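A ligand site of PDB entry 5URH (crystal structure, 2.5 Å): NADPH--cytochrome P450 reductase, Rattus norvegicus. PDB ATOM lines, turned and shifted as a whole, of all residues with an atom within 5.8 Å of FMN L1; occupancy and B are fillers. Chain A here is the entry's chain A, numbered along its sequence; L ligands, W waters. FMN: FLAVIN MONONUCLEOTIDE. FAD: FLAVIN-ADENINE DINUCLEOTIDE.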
ATOM      1  N   GLY A  29       9.337  -7.593  -9.308  1.00  0.00           N
ATOM      2  CA  GLY A  29       9.677  -6.505 -10.202  1.00  0.00           C
ATOM      3  C   GLY A  29       8.682  -6.758 -11.315  1.00  0.00           C
ATOM      4  O   GLY A  29       8.915  -7.577 -12.208  1.00  0.00           O
ATOM      5  N   SER A  30       7.559  -6.063 -11.259  1.00  0.00           N
ATOM      6  CA  SER A  30       6.504  -6.261 -12.251  1.00  0.00           C
ATOM      7  C   SER A  30       5.913  -4.975 -12.788  1.00  0.00           C
ATOM      8  O   SER A  30       5.808  -3.974 -12.081  1.00  0.00           O
ATOM      9  CB  SER A  30       5.397  -7.115 -11.612  1.00  0.00           C
ATOM     10  OG  SER A  30       4.289  -7.275 -12.466  1.00  0.00           O
ATOM     11  N   GLN A  31       5.505  -5.009 -14.047  1.00  0.00           N
ATOM     12  CA  GLN A  31       4.897  -3.840 -14.673  1.00  0.00           C
ATOM     13  C   GLN A  31       3.478  -4.198 -15.118  1.00  0.00           C
ATOM     14  O   GLN A  31       2.532  -3.495 -14.804  1.00  0.00           O
ATOM     15  CB  GLN A  31       5.735  -3.406 -15.876  1.00  0.00           C
ATOM     16  CG  GLN A  31       5.587  -1.958 -16.261  1.00  0.00           C
ATOM     17  CD  GLN A  31       6.894  -1.393 -16.763  1.00  0.00           C
ATOM     18  OE1 GLN A  31       7.890  -1.355 -16.025  1.00  0.00           O
ATOM     19  NE2 GLN A  31       6.915  -0.942 -18.018  1.00  0.00           N
ATOM     20  N   THR A  32       3.342  -5.326 -15.822  1.00  0.00           N
ATOM     21  CA  THR A  32       2.058  -5.792 -16.320  1.00  0.00           C
ATOM     22  C   THR A  32       1.403  -6.766 -15.333  1.00  0.00           C
ATOM     23  O   THR A  32       0.397  -7.399 -15.628  1.00  0.00           O
ATOM     24  CB  THR A  32       2.220  -6.464 -17.696  1.00  0.00           C
ATOM     25  OG1 THR A  32       2.977  -5.588 -18.551  1.00  0.00           O
ATOM     26  CG2 THR A  32       0.870  -6.712 -18.344  1.00  0.00           C
ATOM     27  N   GLY A  33       2.011  -6.898 -14.157  1.00  0.00           N
ATOM     28  CA  GLY A  33       1.433  -7.756 -13.135  1.00  0.00           C
ATOM     29  C   GLY A  33       1.753  -9.244 -13.104  1.00  0.00           C
ATOM     30  O   GLY A  33       1.323  -9.924 -12.176  1.00  0.00           O
ATOM     31  N   THR A  34       2.495  -9.752 -14.086  1.00  0.00           N
ATOM     32  CA  THR A  34       2.804 -11.175 -14.082  1.00  0.00           C
ATOM     33  C   THR A  34       3.678 -11.600 -12.897  1.00  0.00           C
ATOM     34  O   THR A  34       3.313 -12.512 -12.139  1.00  0.00           O
ATOM     35  CB  THR A  34       3.496 -11.619 -15.402  1.00  0.00           C
ATOM     36  OG1 THR A  34       2.761 -11.125 -16.533  1.00  0.00           O
ATOM     37  CG2 THR A  34       3.542 -13.160 -15.479  1.00  0.00           C
ATOM     38  N   ALA A  35       4.818 -10.939 -12.717  1.00  0.00           N
ATOM     39  CA  ALA A  35       5.737 -11.269 -11.636  1.00  0.00           C
ATOM     40  C   ALA A  35       5.068 -11.164 -10.270  1.00  0.00           C
ATOM     41  O   ALA A  35       5.369 -11.928  -9.357  1.00  0.00           O
ATOM     42  CB  ALA A  35       6.960 -10.371 -11.683  1.00  0.00           C
ATOM     43  N   GLU A  36       4.162 -10.201 -10.145  1.00  0.00           N
ATOM     44  CA  GLU A  36       3.460  -9.992  -8.890  1.00  0.00           C
ATOM     45  C   GLU A  36       2.617 -11.222  -8.622  1.00  0.00           C
ATOM     46  O   GLU A  36       2.435 -11.626  -7.481  1.00  0.00           O
ATOM     47  CB  GLU A  36       2.550  -8.774  -8.993  1.00  0.00           C
ATOM     48  CG  GLU A  36       2.036  -8.239  -7.675  1.00  0.00           C
ATOM     49  CD  GLU A  36       1.119  -7.044  -7.858  1.00  0.00           C
ATOM     50  OE1 GLU A  36       1.388  -6.238  -8.788  1.00  0.00           O
ATOM     51  OE2 GLU A  36       0.157  -6.897  -7.073  1.00  0.00           O
ATOM     52  N   ALA A  82      11.034  -9.124 -13.653  1.00  0.00           N
ATOM     53  CA  ALA A  82      10.781  -9.032 -15.084  1.00  0.00           C
ATOM     54  C   ALA A  82      11.728  -7.997 -15.659  1.00  0.00           C
ATOM     55  O   ALA A  82      12.199  -7.117 -14.939  1.00  0.00           O
ATOM     56  CB  ALA A  82       9.340  -8.599 -15.335  1.00  0.00           C
ATOM     57  N   THR A  83      12.024  -8.107 -16.952  1.00  0.00           N
ATOM     58  CA  THR A  83      12.915  -7.159 -17.603  1.00  0.00           C
ATOM     59  C   THR A  83      12.162  -6.302 -18.615  1.00  0.00           C
ATOM     60  O   THR A  83      11.271  -6.792 -19.302  1.00  0.00           O
ATOM     61  CB  THR A  83      14.055  -7.871 -18.366  1.00  0.00           C
ATOM     62  OG1 THR A  83      14.754  -8.755 -17.495  1.00  0.00           O
ATOM     63  CG2 THR A  83      15.025  -6.841 -18.914  1.00  0.00           C
ATOM     64  N   TYR A  84      12.527  -5.021 -18.709  1.00  0.00           N
ATOM     65  CA  TYR A  84      11.894  -4.120 -19.672  1.00  0.00           C
ATOM     66  C   TYR A  84      12.875  -3.283 -20.491  1.00  0.00           C
ATOM     67  O   TYR A  84      13.927  -2.897 -20.006  1.00  0.00           O
ATOM     68  CB  TYR A  84      10.888  -3.196 -18.975  1.00  0.00           C
ATOM     69  CG  TYR A  84       9.548  -3.866 -18.754  1.00  0.00           C
ATOM     70  CD1 TYR A  84       9.383  -4.810 -17.740  1.00  0.00           C
ATOM     71  CD2 TYR A  84       8.476  -3.611 -19.607  1.00  0.00           C
ATOM     72  CE1 TYR A  84       8.177  -5.501 -17.584  1.00  0.00           C
ATOM     73  CE2 TYR A  84       7.265  -4.300 -19.464  1.00  0.00           C
ATOM     74  CZ  TYR A  84       7.122  -5.236 -18.448  1.00  0.00           C
ATOM     75  OH  TYR A  84       5.933  -5.921 -18.313  1.00  0.00           O
ATOM     76  N   GLY A  85      12.477  -3.033 -21.737  1.00  0.00           N
ATOM     77  CA  GLY A  85      13.254  -2.256 -22.692  1.00  0.00           C
ATOM     78  C   GLY A  85      14.749  -2.187 -22.426  1.00  0.00           C
ATOM     79  O   GLY A  85      15.185  -1.562 -21.463  1.00  0.00           O
ATOM     80  N   GLU A  86      15.526  -2.814 -23.301  1.00  0.00           N
ATOM     81  CA  GLU A  86      16.986  -2.823 -23.186  1.00  0.00           C
ATOM     82  C   GLU A  86      17.508  -3.378 -21.855  1.00  0.00           C
ATOM     83  O   GLU A  86      18.325  -2.740 -21.183  1.00  0.00           O
ATOM     84  CB  GLU A  86      17.499  -1.398 -23.405  1.00  0.00           C
ATOM     85  N   GLY A  87      17.021  -4.556 -21.497  1.00  0.00           N
ATOM     86  CA  GLY A  87      17.449  -5.193 -20.271  1.00  0.00           C
ATOM     87  C   GLY A  87      17.399  -4.314 -19.040  1.00  0.00           C
ATOM     88  O   GLY A  87      18.308  -4.370 -18.196  1.00  0.00           O
ATOM     89  N   ASP A  88      16.361  -3.504 -18.914  1.00  0.00           N
ATOM     90  CA  ASP A  88      16.243  -2.639 -17.745  1.00  0.00           C
ATOM     91  C   ASP A  88      15.328  -3.224 -16.694  1.00  0.00           C
ATOM     92  O   ASP A  88      14.592  -4.181 -16.957  1.00  0.00           O
ATOM     93  CB  ASP A  88      15.713  -1.261 -18.153  1.00  0.00           C
ATOM     94  CG  ASP A  88      16.791  -0.370 -18.758  1.00  0.00           C
ATOM     95  OD1 ASP A  88      17.847  -0.177 -18.100  1.00  0.00           O
ATOM     96  OD2 ASP A  88      16.572   0.137 -19.884  1.00  0.00           O
ATOM     97  N   THR A  90      12.143  -3.196 -14.000  1.00  0.00           N
ATOM     98  CA  THR A  90      10.798  -2.657 -14.079  1.00  0.00           C
ATOM     99  C   THR A  90      10.878  -1.374 -13.249  1.00  0.00           C
ATOM    100  O   THR A  90      11.732  -1.263 -12.370  1.00  0.00           O
ATOM    101  CB  THR A  90       9.765  -3.610 -13.475  1.00  0.00           C
ATOM    102  OG1 THR A  90      10.106  -3.895 -12.107  1.00  0.00           O
ATOM    103  CG2 THR A  90       9.727  -4.900 -14.261  1.00  0.00           C
ATOM    104  N   LEU A 117      11.483 -13.234 -15.282  1.00  0.00           N
ATOM    105  CA  LEU A 117      10.469 -13.236 -16.331  1.00  0.00           C
ATOM    106  C   LEU A 117      11.007 -12.419 -17.487  1.00  0.00           C
ATOM    107  O   LEU A 117      11.409 -11.261 -17.321  1.00  0.00           O
ATOM    108  CB  LEU A 117       9.165 -12.595 -15.854  1.00  0.00           C
ATOM    109  CG  LEU A 117       8.341 -13.335 -14.803  1.00  0.00           C
ATOM    110  CD1 LEU A 117       9.025 -13.234 -13.441  1.00  0.00           C
ATOM    111  CD2 LEU A 117       6.956 -12.730 -14.751  1.00  0.00           C
ATOM    112  N   GLY A 118      11.019 -13.014 -18.670  1.00  0.00           N
ATOM    113  CA  GLY A 118      11.506 -12.323 -19.842  1.00  0.00           C
ATOM    114  C   GLY A 118      10.891 -12.873 -21.107  1.00  0.00           C
ATOM    115  O   GLY A 118       9.858 -13.536 -21.080  1.00  0.00           O
ATOM    116  N   ASN A 119      11.548 -12.599 -22.229  1.00  0.00           N
ATOM    117  CA  ASN A 119      11.072 -13.053 -23.525  1.00  0.00           C
ATOM    118  C   ASN A 119      12.286 -13.153 -24.443  1.00  0.00           C
ATOM    119  O   ASN A 119      12.965 -12.154 -24.675  1.00  0.00           O
ATOM    120  CB  ASN A 119      10.063 -12.062 -24.082  1.00  0.00           C
ATOM    121  CG  ASN A 119       9.505 -12.492 -25.403  1.00  0.00           C
ATOM    122  OD1 ASN A 119      10.218 -13.113 -26.206  1.00  0.00           O
ATOM    123  ND2 ASN A 119       8.246 -12.164 -25.656  1.00  0.00           N
ATOM    124  N   LYS A 120      12.540 -14.340 -24.985  1.00  0.00           N
ATOM    125  CA  LYS A 120      13.691 -14.554 -25.850  1.00  0.00           C
ATOM    126  C   LYS A 120      13.839 -13.663 -27.086  1.00  0.00           C
ATOM    127  O   LYS A 120      14.952 -13.411 -27.538  1.00  0.00           O
ATOM    128  CB  LYS A 120      13.763 -16.014 -26.290  1.00  0.00           C
ATOM    129  CG  LYS A 120      14.254 -16.962 -25.206  1.00  0.00           C
ATOM    130  CD  LYS A 120      14.484 -18.364 -25.779  1.00  0.00           C
ATOM    131  CE  LYS A 120      15.105 -19.297 -24.741  1.00  0.00           C
ATOM    132  NZ  LYS A 120      14.230 -19.458 -23.541  1.00  0.00           N
ATOM    133  N   TYR A 122      14.030 -10.755 -27.453  1.00  0.00           N
ATOM    134  CA  TYR A 122      14.632  -9.471 -27.135  1.00  0.00           C
ATOM    135  C   TYR A 122      16.157  -9.604 -27.003  1.00  0.00           C
ATOM    136  O   TYR A 122      16.667 -10.692 -26.731  1.00  0.00           O
ATOM    137  CB  TYR A 122      14.063  -8.884 -25.846  1.00  0.00           C
ATOM    138  CG  TYR A 122      12.631  -8.378 -25.961  1.00  0.00           C
ATOM    139  CD1 TYR A 122      11.553  -9.256 -25.927  1.00  0.00           C
ATOM    140  CD2 TYR A 122      12.371  -7.017 -26.106  1.00  0.00           C
ATOM    141  CE1 TYR A 122      10.236  -8.796 -26.035  1.00  0.00           C
ATOM    142  CE2 TYR A 122      11.060  -6.534 -26.211  1.00  0.00           C
ATOM    143  CZ  TYR A 122      10.002  -7.431 -26.165  1.00  0.00           C
ATOM    144  OH  TYR A 122       8.699  -6.971 -26.271  1.00  0.00           O
ATOM    145  N   GLU A 123      16.863  -8.497 -27.206  1.00  0.00           N
ATOM    146  CA  GLU A 123      18.314  -8.473 -27.127  1.00  0.00           C
ATOM    147  C   GLU A 123      18.824  -9.062 -25.806  1.00  0.00           C
ATOM    148  O   GLU A 123      19.406 -10.153 -25.780  1.00  0.00           O
ATOM    149  CB  GLU A 123      18.829  -7.039 -27.283  1.00  0.00           C
ATOM    150  N   HIS A 124      18.574  -8.335 -24.718  1.00  0.00           N
ATOM    151  CA  HIS A 124      19.001  -8.763 -23.399  1.00  0.00           C
ATOM    152  C   HIS A 124      17.931  -9.614 -22.688  1.00  0.00           C
ATOM    153  O   HIS A 124      17.175  -9.121 -21.867  1.00  0.00           O
ATOM    154  CB  HIS A 124      19.325  -7.530 -22.558  1.00  0.00           C
ATOM    155  CG  HIS A 124      20.164  -6.528 -23.293  1.00  0.00           C
ATOM    156  ND1 HIS A 124      19.695  -5.823 -24.379  1.00  0.00           N
ATOM    157  CD2 HIS A 124      21.441  -6.127 -23.109  1.00  0.00           C
ATOM    158  CE1 HIS A 124      20.641  -5.028 -24.830  1.00  0.00           C
ATOM    159  NE2 HIS A 124      21.715  -5.189 -24.089  1.00  0.00           N
ATOM    160  N   PHE A 125      17.909 -10.897 -23.029  1.00  0.00           N
ATOM    161  CA  PHE A 125      16.960 -11.842 -22.455  1.00  0.00           C
ATOM    162  C   PHE A 125      17.107 -11.999 -20.944  1.00  0.00           C
ATOM    163  O   PHE A 125      18.159 -12.386 -20.446  1.00  0.00           O
ATOM    164  CB  PHE A 125      17.130 -13.202 -23.144  1.00  0.00           C
ATOM    165  CG  PHE A 125      16.377 -14.306 -22.473  1.00  0.00           C
ATOM    166  CD1 PHE A 125      14.986 -14.278 -22.408  1.00  0.00           C
ATOM    167  CD2 PHE A 125      17.053 -15.386 -21.923  1.00  0.00           C
ATOM    168  CE1 PHE A 125      14.283 -15.299 -21.792  1.00  0.00           C
ATOM    169  CE2 PHE A 125      16.364 -16.420 -21.299  1.00  0.00           C
ATOM    170  CZ  PHE A 125      14.978 -16.381 -21.227  1.00  0.00           C
ATOM    171  N   ASN A 126      16.041 -11.692 -20.208  1.00  0.00           N
ATOM    172  CA  ASN A 126      16.045 -11.794 -18.745  1.00  0.00           C
ATOM    173  C   ASN A 126      17.191 -11.099 -18.033  1.00  0.00           C
ATOM    174  O   ASN A 126      17.596 -11.533 -16.955  1.00  0.00           O
ATOM    175  CB  ASN A 126      16.014 -13.265 -18.319  1.00  0.00           C
ATOM    176  CG  ASN A 126      14.632 -13.729 -17.935  1.00  0.00           C
ATOM    177  OD1 ASN A 126      14.045 -13.228 -16.976  1.00  0.00           O
ATOM    178  ND2 ASN A 126      14.103 -14.685 -18.681  1.00  0.00           N
ATOM    179  N   ALA A 127      17.697 -10.009 -18.604  1.00  0.00           N
ATOM    180  CA  ALA A 127      18.805  -9.282 -18.010  1.00  0.00           C
ATOM    181  C   ALA A 127      18.633  -8.974 -16.519  1.00  0.00           C
ATOM    182  O   ALA A 127      19.569  -9.170 -15.725  1.00  0.00           O
ATOM    183  CB  ALA A 127      19.030  -7.990 -18.776  1.00  0.00           C
ATOM    184  N   ASP A 152       8.595 -15.856 -21.987  1.00  0.00           N
ATOM    185  CA  ASP A 152       7.252 -15.481 -22.383  1.00  0.00           C
ATOM    186  C   ASP A 152       6.960 -15.707 -23.862  1.00  0.00           C
ATOM    187  O   ASP A 152       5.804 -15.621 -24.286  1.00  0.00           O
ATOM    188  CB  ASP A 152       6.993 -14.014 -22.024  1.00  0.00           C
ATOM    189  CG  ASP A 152       5.521 -13.640 -22.052  1.00  0.00           C
ATOM    190  OD1 ASP A 152       4.691 -14.468 -21.599  1.00  0.00           O
ATOM    191  OD2 ASP A 152       5.189 -12.526 -22.518  1.00  0.00           O
ATOM    192  N   LEU A 156       5.591 -18.872 -20.402  1.00  0.00           N
ATOM    193  CA  LEU A 156       6.096 -18.464 -19.104  1.00  0.00           C
ATOM    194  C   LEU A 156       5.466 -19.260 -17.962  1.00  0.00           C
ATOM    195  O   LEU A 156       6.168 -19.717 -17.058  1.00  0.00           O
ATOM    196  CB  LEU A 156       5.836 -16.968 -18.908  1.00  0.00           C
ATOM    197  CG  LEU A 156       6.357 -16.356 -17.609  1.00  0.00           C
ATOM    198  CD1 LEU A 156       7.875 -16.482 -17.558  1.00  0.00           C
ATOM    199  CD2 LEU A 156       5.934 -14.902 -17.538  1.00  0.00           C
ATOM    200  N   VAL A 620       9.502  -2.371 -30.190  1.00  0.00           N
ATOM    201  CA  VAL A 620       8.756  -3.534 -30.603  1.00  0.00           C
ATOM    202  C   VAL A 620       7.827  -3.992 -29.495  1.00  0.00           C
ATOM    203  O   VAL A 620       8.071  -3.754 -28.312  1.00  0.00           O
ATOM    204  CB  VAL A 620       9.688  -4.699 -30.962  1.00  0.00           C
ATOM    205  CG1 VAL A 620      10.530  -4.329 -32.172  1.00  0.00           C
ATOM    206  CG2 VAL A 620      10.563  -5.021 -29.761  1.00  0.00           C
HETATM  207  N1  FMN L   1      11.935  -9.408 -21.841  1.00  0.00           N
HETATM  208  C2  FMN L   1      13.266  -9.606 -21.819  1.00  0.00           C
HETATM  209  O2  FMN L   1      13.753 -10.710 -21.535  1.00  0.00           O
HETATM  210  N3  FMN L   1      14.067  -8.518 -22.149  1.00  0.00           N
HETATM  211  C4  FMN L   1      13.645  -7.231 -22.502  1.00  0.00           C
HETATM  212  O4  FMN L   1      14.548  -6.426 -22.748  1.00  0.00           O
HETATM  213  C4A FMN L   1      12.235  -7.008 -22.527  1.00  0.00           C
HETATM  214  N5  FMN L   1      11.764  -5.715 -22.891  1.00  0.00           N
HETATM  215  C5A FMN L   1      10.362  -5.602 -22.905  1.00  0.00           C
HETATM  216  C6  FMN L   1       9.837  -4.314 -23.288  1.00  0.00           C
HETATM  217  C7  FMN L   1       8.447  -4.062 -23.353  1.00  0.00           C
HETATM  218  C7M FMN L   1       8.034  -2.635 -23.779  1.00  0.00           C
HETATM  219  C8  FMN L   1       7.465  -5.147 -23.015  1.00  0.00           C
HETATM  220  C8M FMN L   1       6.088  -5.034 -23.046  1.00  0.00           C
HETATM  221  C9  FMN L   1       7.948  -6.393 -22.644  1.00  0.00           C
HETATM  222  C9A FMN L   1       9.389  -6.670 -22.582  1.00  0.00           C
HETATM  223  N10 FMN L   1       9.973  -7.977 -22.202  1.00  0.00           N
HETATM  224  C10 FMN L   1      11.440  -8.158 -22.183  1.00  0.00           C
HETATM  225  C1' FMN L   1       9.119  -9.091 -21.851  1.00  0.00           C
HETATM  226  C2' FMN L   1       8.718  -9.113 -20.353  1.00  0.00           C
HETATM  227  O2' FMN L   1       9.959  -9.204 -19.552  1.00  0.00           O
HETATM  228  C3' FMN L   1       7.809 -10.301 -20.082  1.00  0.00           C
HETATM  229  O3' FMN L   1       6.625 -10.111 -20.898  1.00  0.00           O
HETATM  230  C4' FMN L   1       7.440 -10.320 -18.557  1.00  0.00           C
HETATM  231  O4' FMN L   1       6.635 -11.528 -18.508  1.00  0.00           O
HETATM  232  C5' FMN L   1       6.503  -9.211 -18.124  1.00  0.00           C
HETATM  233  O5' FMN L   1       6.214  -9.270 -16.678  1.00  0.00           O
HETATM  234  P   FMN L   1       5.232  -8.323 -15.877  1.00  0.00           P
HETATM  235  O1P FMN L   1       3.836  -8.600 -16.305  1.00  0.00           O
HETATM  236  O2P FMN L   1       5.838  -6.900 -16.056  1.00  0.00           O
HETATM  237  O3P FMN L   1       5.422  -8.892 -14.374  1.00  0.00           O
HETATM  238  PA  FAD L   2      -6.128  -7.997 -25.724  1.00  0.00           P
HETATM  239  O1A FAD L   2      -7.407  -8.264 -25.026  1.00  0.00           O
HETATM  240  O2A FAD L   2      -4.975  -7.501 -24.936  1.00  0.00           O
HETATM  241  O5B FAD L   2      -5.678  -9.331 -26.499  1.00  0.00           O
HETATM  242  C5B FAD L   2      -4.384  -9.385 -27.105  1.00  0.00           C
HETATM  243  C4B FAD L   2      -3.967 -10.849 -27.261  1.00  0.00           C
HETATM  244  O4B FAD L   2      -4.816 -11.531 -28.193  1.00  0.00           O
HETATM  245  C3B FAD L   2      -2.611 -10.949 -27.924  1.00  0.00           C
HETATM  246  O3B FAD L   2      -1.608 -10.656 -26.945  1.00  0.00           O
HETATM  247  C2B FAD L   2      -2.629 -12.435 -28.219  1.00  0.00           C
HETATM  248  O2B FAD L   2      -2.360 -13.156 -27.013  1.00  0.00           O
HETATM  249  C1B FAD L   2      -4.060 -12.663 -28.662  1.00  0.00           C
HETATM  250  N9A FAD L   2      -4.179 -12.662 -30.141  1.00  0.00           N
HETATM  251  C8A FAD L   2      -4.132 -11.481 -31.018  1.00  0.00           C
HETATM  252  N7A FAD L   2      -4.474 -12.104 -32.311  1.00  0.00           N
HETATM  253  C5A FAD L   2      -4.528 -13.423 -32.144  1.00  0.00           C
HETATM  254  C6A FAD L   2      -4.801 -14.382 -33.036  1.00  0.00           C
HETATM  255  N6A FAD L   2      -5.114 -13.969 -34.263  1.00  0.00           N
HETATM  256  N1A FAD L   2      -4.750 -15.684 -32.736  1.00  0.00           N
HETATM  257  C2A FAD L   2      -4.379 -16.057 -31.437  1.00  0.00           C
HETATM  258  N3A FAD L   2      -4.090 -15.037 -30.522  1.00  0.00           N
HETATM  259  C4A FAD L   2      -4.184 -13.747 -30.902  1.00  0.00           C
HETATM  260  N1  FAD L   2      -0.699  -1.610 -30.683  1.00  0.00           N
HETATM  261  C2  FAD L   2      -1.128  -0.779 -31.732  1.00  0.00           C
HETATM  262  O2  FAD L   2      -2.038  -1.141 -32.461  1.00  0.00           O
HETATM  263  N3  FAD L   2      -0.509   0.467 -31.917  1.00  0.00           N
HETATM  264  C4  FAD L   2       0.523   0.881 -31.077  1.00  0.00           C
HETATM  265  O4  FAD L   2       0.948   2.028 -31.163  1.00  0.00           O
HETATM  266  C4X FAD L   2       0.957   0.040 -30.055  1.00  0.00           C
HETATM  267  N5  FAD L   2       2.070   0.339 -29.373  1.00  0.00           N
HETATM  268  C5X FAD L   2       2.488  -0.477 -28.385  1.00  0.00           C
HETATM  269  C6  FAD L   2       3.583  -0.113 -27.612  1.00  0.00           C
HETATM  270  C7  FAD L   2       4.007  -0.940 -26.575  1.00  0.00           C
HETATM  271  C7M FAD L   2       5.132  -0.600 -25.841  1.00  0.00           C
HETATM  272  C8  FAD L   2       3.304  -2.110 -26.294  1.00  0.00           C
HETATM  273  C8M FAD L   2       3.702  -2.921 -25.235  1.00  0.00           C
HETATM  274  C9  FAD L   2       2.190  -2.450 -27.047  1.00  0.00           C
HETATM  275  C9A FAD L   2       1.764  -1.619 -28.075  1.00  0.00           C
HETATM  276  N10 FAD L   2       0.626  -1.888 -28.740  1.00  0.00           N
HETATM  277  C10 FAD L   2       0.339  -1.189 -29.844  1.00  0.00           C
HETATM  278  C1' FAD L   2      -0.186  -3.083 -28.415  1.00  0.00           C
HETATM  279  C2' FAD L   2      -1.327  -2.716 -27.466  1.00  0.00           C
HETATM  280  O2' FAD L   2      -0.791  -2.249 -26.229  1.00  0.00           O
HETATM  281  C3' FAD L   2      -2.269  -3.889 -27.217  1.00  0.00           C
HETATM  282  O3' FAD L   2      -1.514  -5.058 -26.857  1.00  0.00           O
HETATM  283  C4' FAD L   2      -3.119  -4.171 -28.454  1.00  0.00           C
HETATM  284  O4' FAD L   2      -3.829  -2.995 -28.830  1.00  0.00           O
HETATM  285  C5' FAD L   2      -4.106  -5.304 -28.164  1.00  0.00           C
HETATM  286  O5' FAD L   2      -4.790  -5.033 -26.940  1.00  0.00           O
HETATM  287  P   FAD L   2      -6.345  -5.379 -26.742  1.00  0.00           P
HETATM  288  O1P FAD L   2      -7.128  -4.752 -27.824  1.00  0.00           O
HETATM  289  O2P FAD L   2      -6.696  -5.044 -25.338  1.00  0.00           O
HETATM  290  O3P FAD L   2      -6.405  -6.976 -26.937  1.00  0.00           O
HETATM  291  O   HOH W   1       4.551  -8.179 -21.080  1.00  0.00           O
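O2 of FMN L1 lies within hydrogen-bond range of N of Asn 119.
O of Leu 117 sits at hydrogen-bond distance from O2' of FMN L1 (3.4 Å).
N of Ala 35 is in hydrogen-bond range of O3P of FMN L1.
The side-chain hydroxyl (OG1) of Thr 34 lies within hydrogen-bond range of an oxygen (O1P) of FMN L1.
O of Thr 83 lies within hydrogen-bond range of O2' of FMN L1 (2.8 Å).
O of His 124 sits at hydrogen-bond distance from N3 of FMN L1 (3.2 Å).
N of Gln 31 sits at hydrogen-bond distance from O2P of FMN L1 (2.8 Å).
The side-chain hydroxyl (OH) of Tyr 84 is in hydrogen-bond range of an oxygen (O2P) of FMN L1 (2.5 Å).
The side-chain carboxylate (OD2) of Asp 152 is in hydrogen-bond range of an oxygen (O3') of FMN L1 (3.2 Å).
N of Gly 87 is in hydrogen-bond range of O4 of FMN L1 (3.3 Å).
An oxygen (O2P) of FMN L1 is in hydrogen-bond range of the backbone NH (N) of Thr 32 (3.0 Å).
N of Asn 126 is in hydrogen-bond range of O2 of FMN L1 (2.8 Å).
O2' of FMN L1 is in hydrogen-bond range of N of Thr 83 (3.5 Å).
An oxygen (O1P) of FMN L1 is in hydrogen-bond range of the backbone NH (N) of Thr 34.
N of Gly 85 is in hydrogen-bond range of N5 of FMN L1 (3.0 Å).
The backbone NH of Gly 33 is in hydrogen-bond range of an oxygen (O1P) of FMN L1 (3.3 Å).
The side-chain hydroxyl (OG) of Ser 30 lies within hydrogen-bond range of an oxygen (O3P) of FMN L1 (2.7 Å).
N of Ala 82 sits at hydrogen-bond distance from O of Gly 29.
The side-chain amide oxygen (OD1) of Asn 126 is in hydrogen-bond range of the backbone NH (N) of Gly 118.
The backbone carbonyl oxygen (O) of Gly 118 is in hydrogen-bond range of the backbone NH (N) of Asp 152.
The backbone NH (N) of Thr 83 is in hydrogen-bond range of the backbone carbonyl oxygen (O) of Leu 117 (3.2 Å).
O of Gly 85 lies close to OD2 of Asp 88 (2.7 Å).
OG of Ser 30 lies within hydrogen-bond range of N of Gly 33 (2.9 Å).
OG1 of Thr 90 is in hydrogen-bond range of N of Ser 30 (3.5 Å).
OD1 of Asn 126 sits at hydrogen-bond distance from N of Leu 117 (3.1 Å).
Ala 82 touches FMN L1.
Glu 86 touches FMN L1 (N to O4, 3.8 Å).
Gly 118 touches FMN L1 (CA to O2, 3.2 Å).
Tyr 122 touches FMN L1 (CE2 to N5, 3.5 Å).
Phe 125 touches FMN L1 (CA to O2, 3.5 Å).
Leu 156 touches FMN L1.
Hydrophobic or aromatic side chains within 4 Å of FMN L1: Ala 35, Ala 82, Tyr 84, Leu 117, Tyr 122, Phe 125 and Leu 156.
Along chain A the residues within 4 Å of FMN L1 span positions 30 to 156.
The nearest printed residue that does not touch FMN L1 is Gly 29 (4.3 Å).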
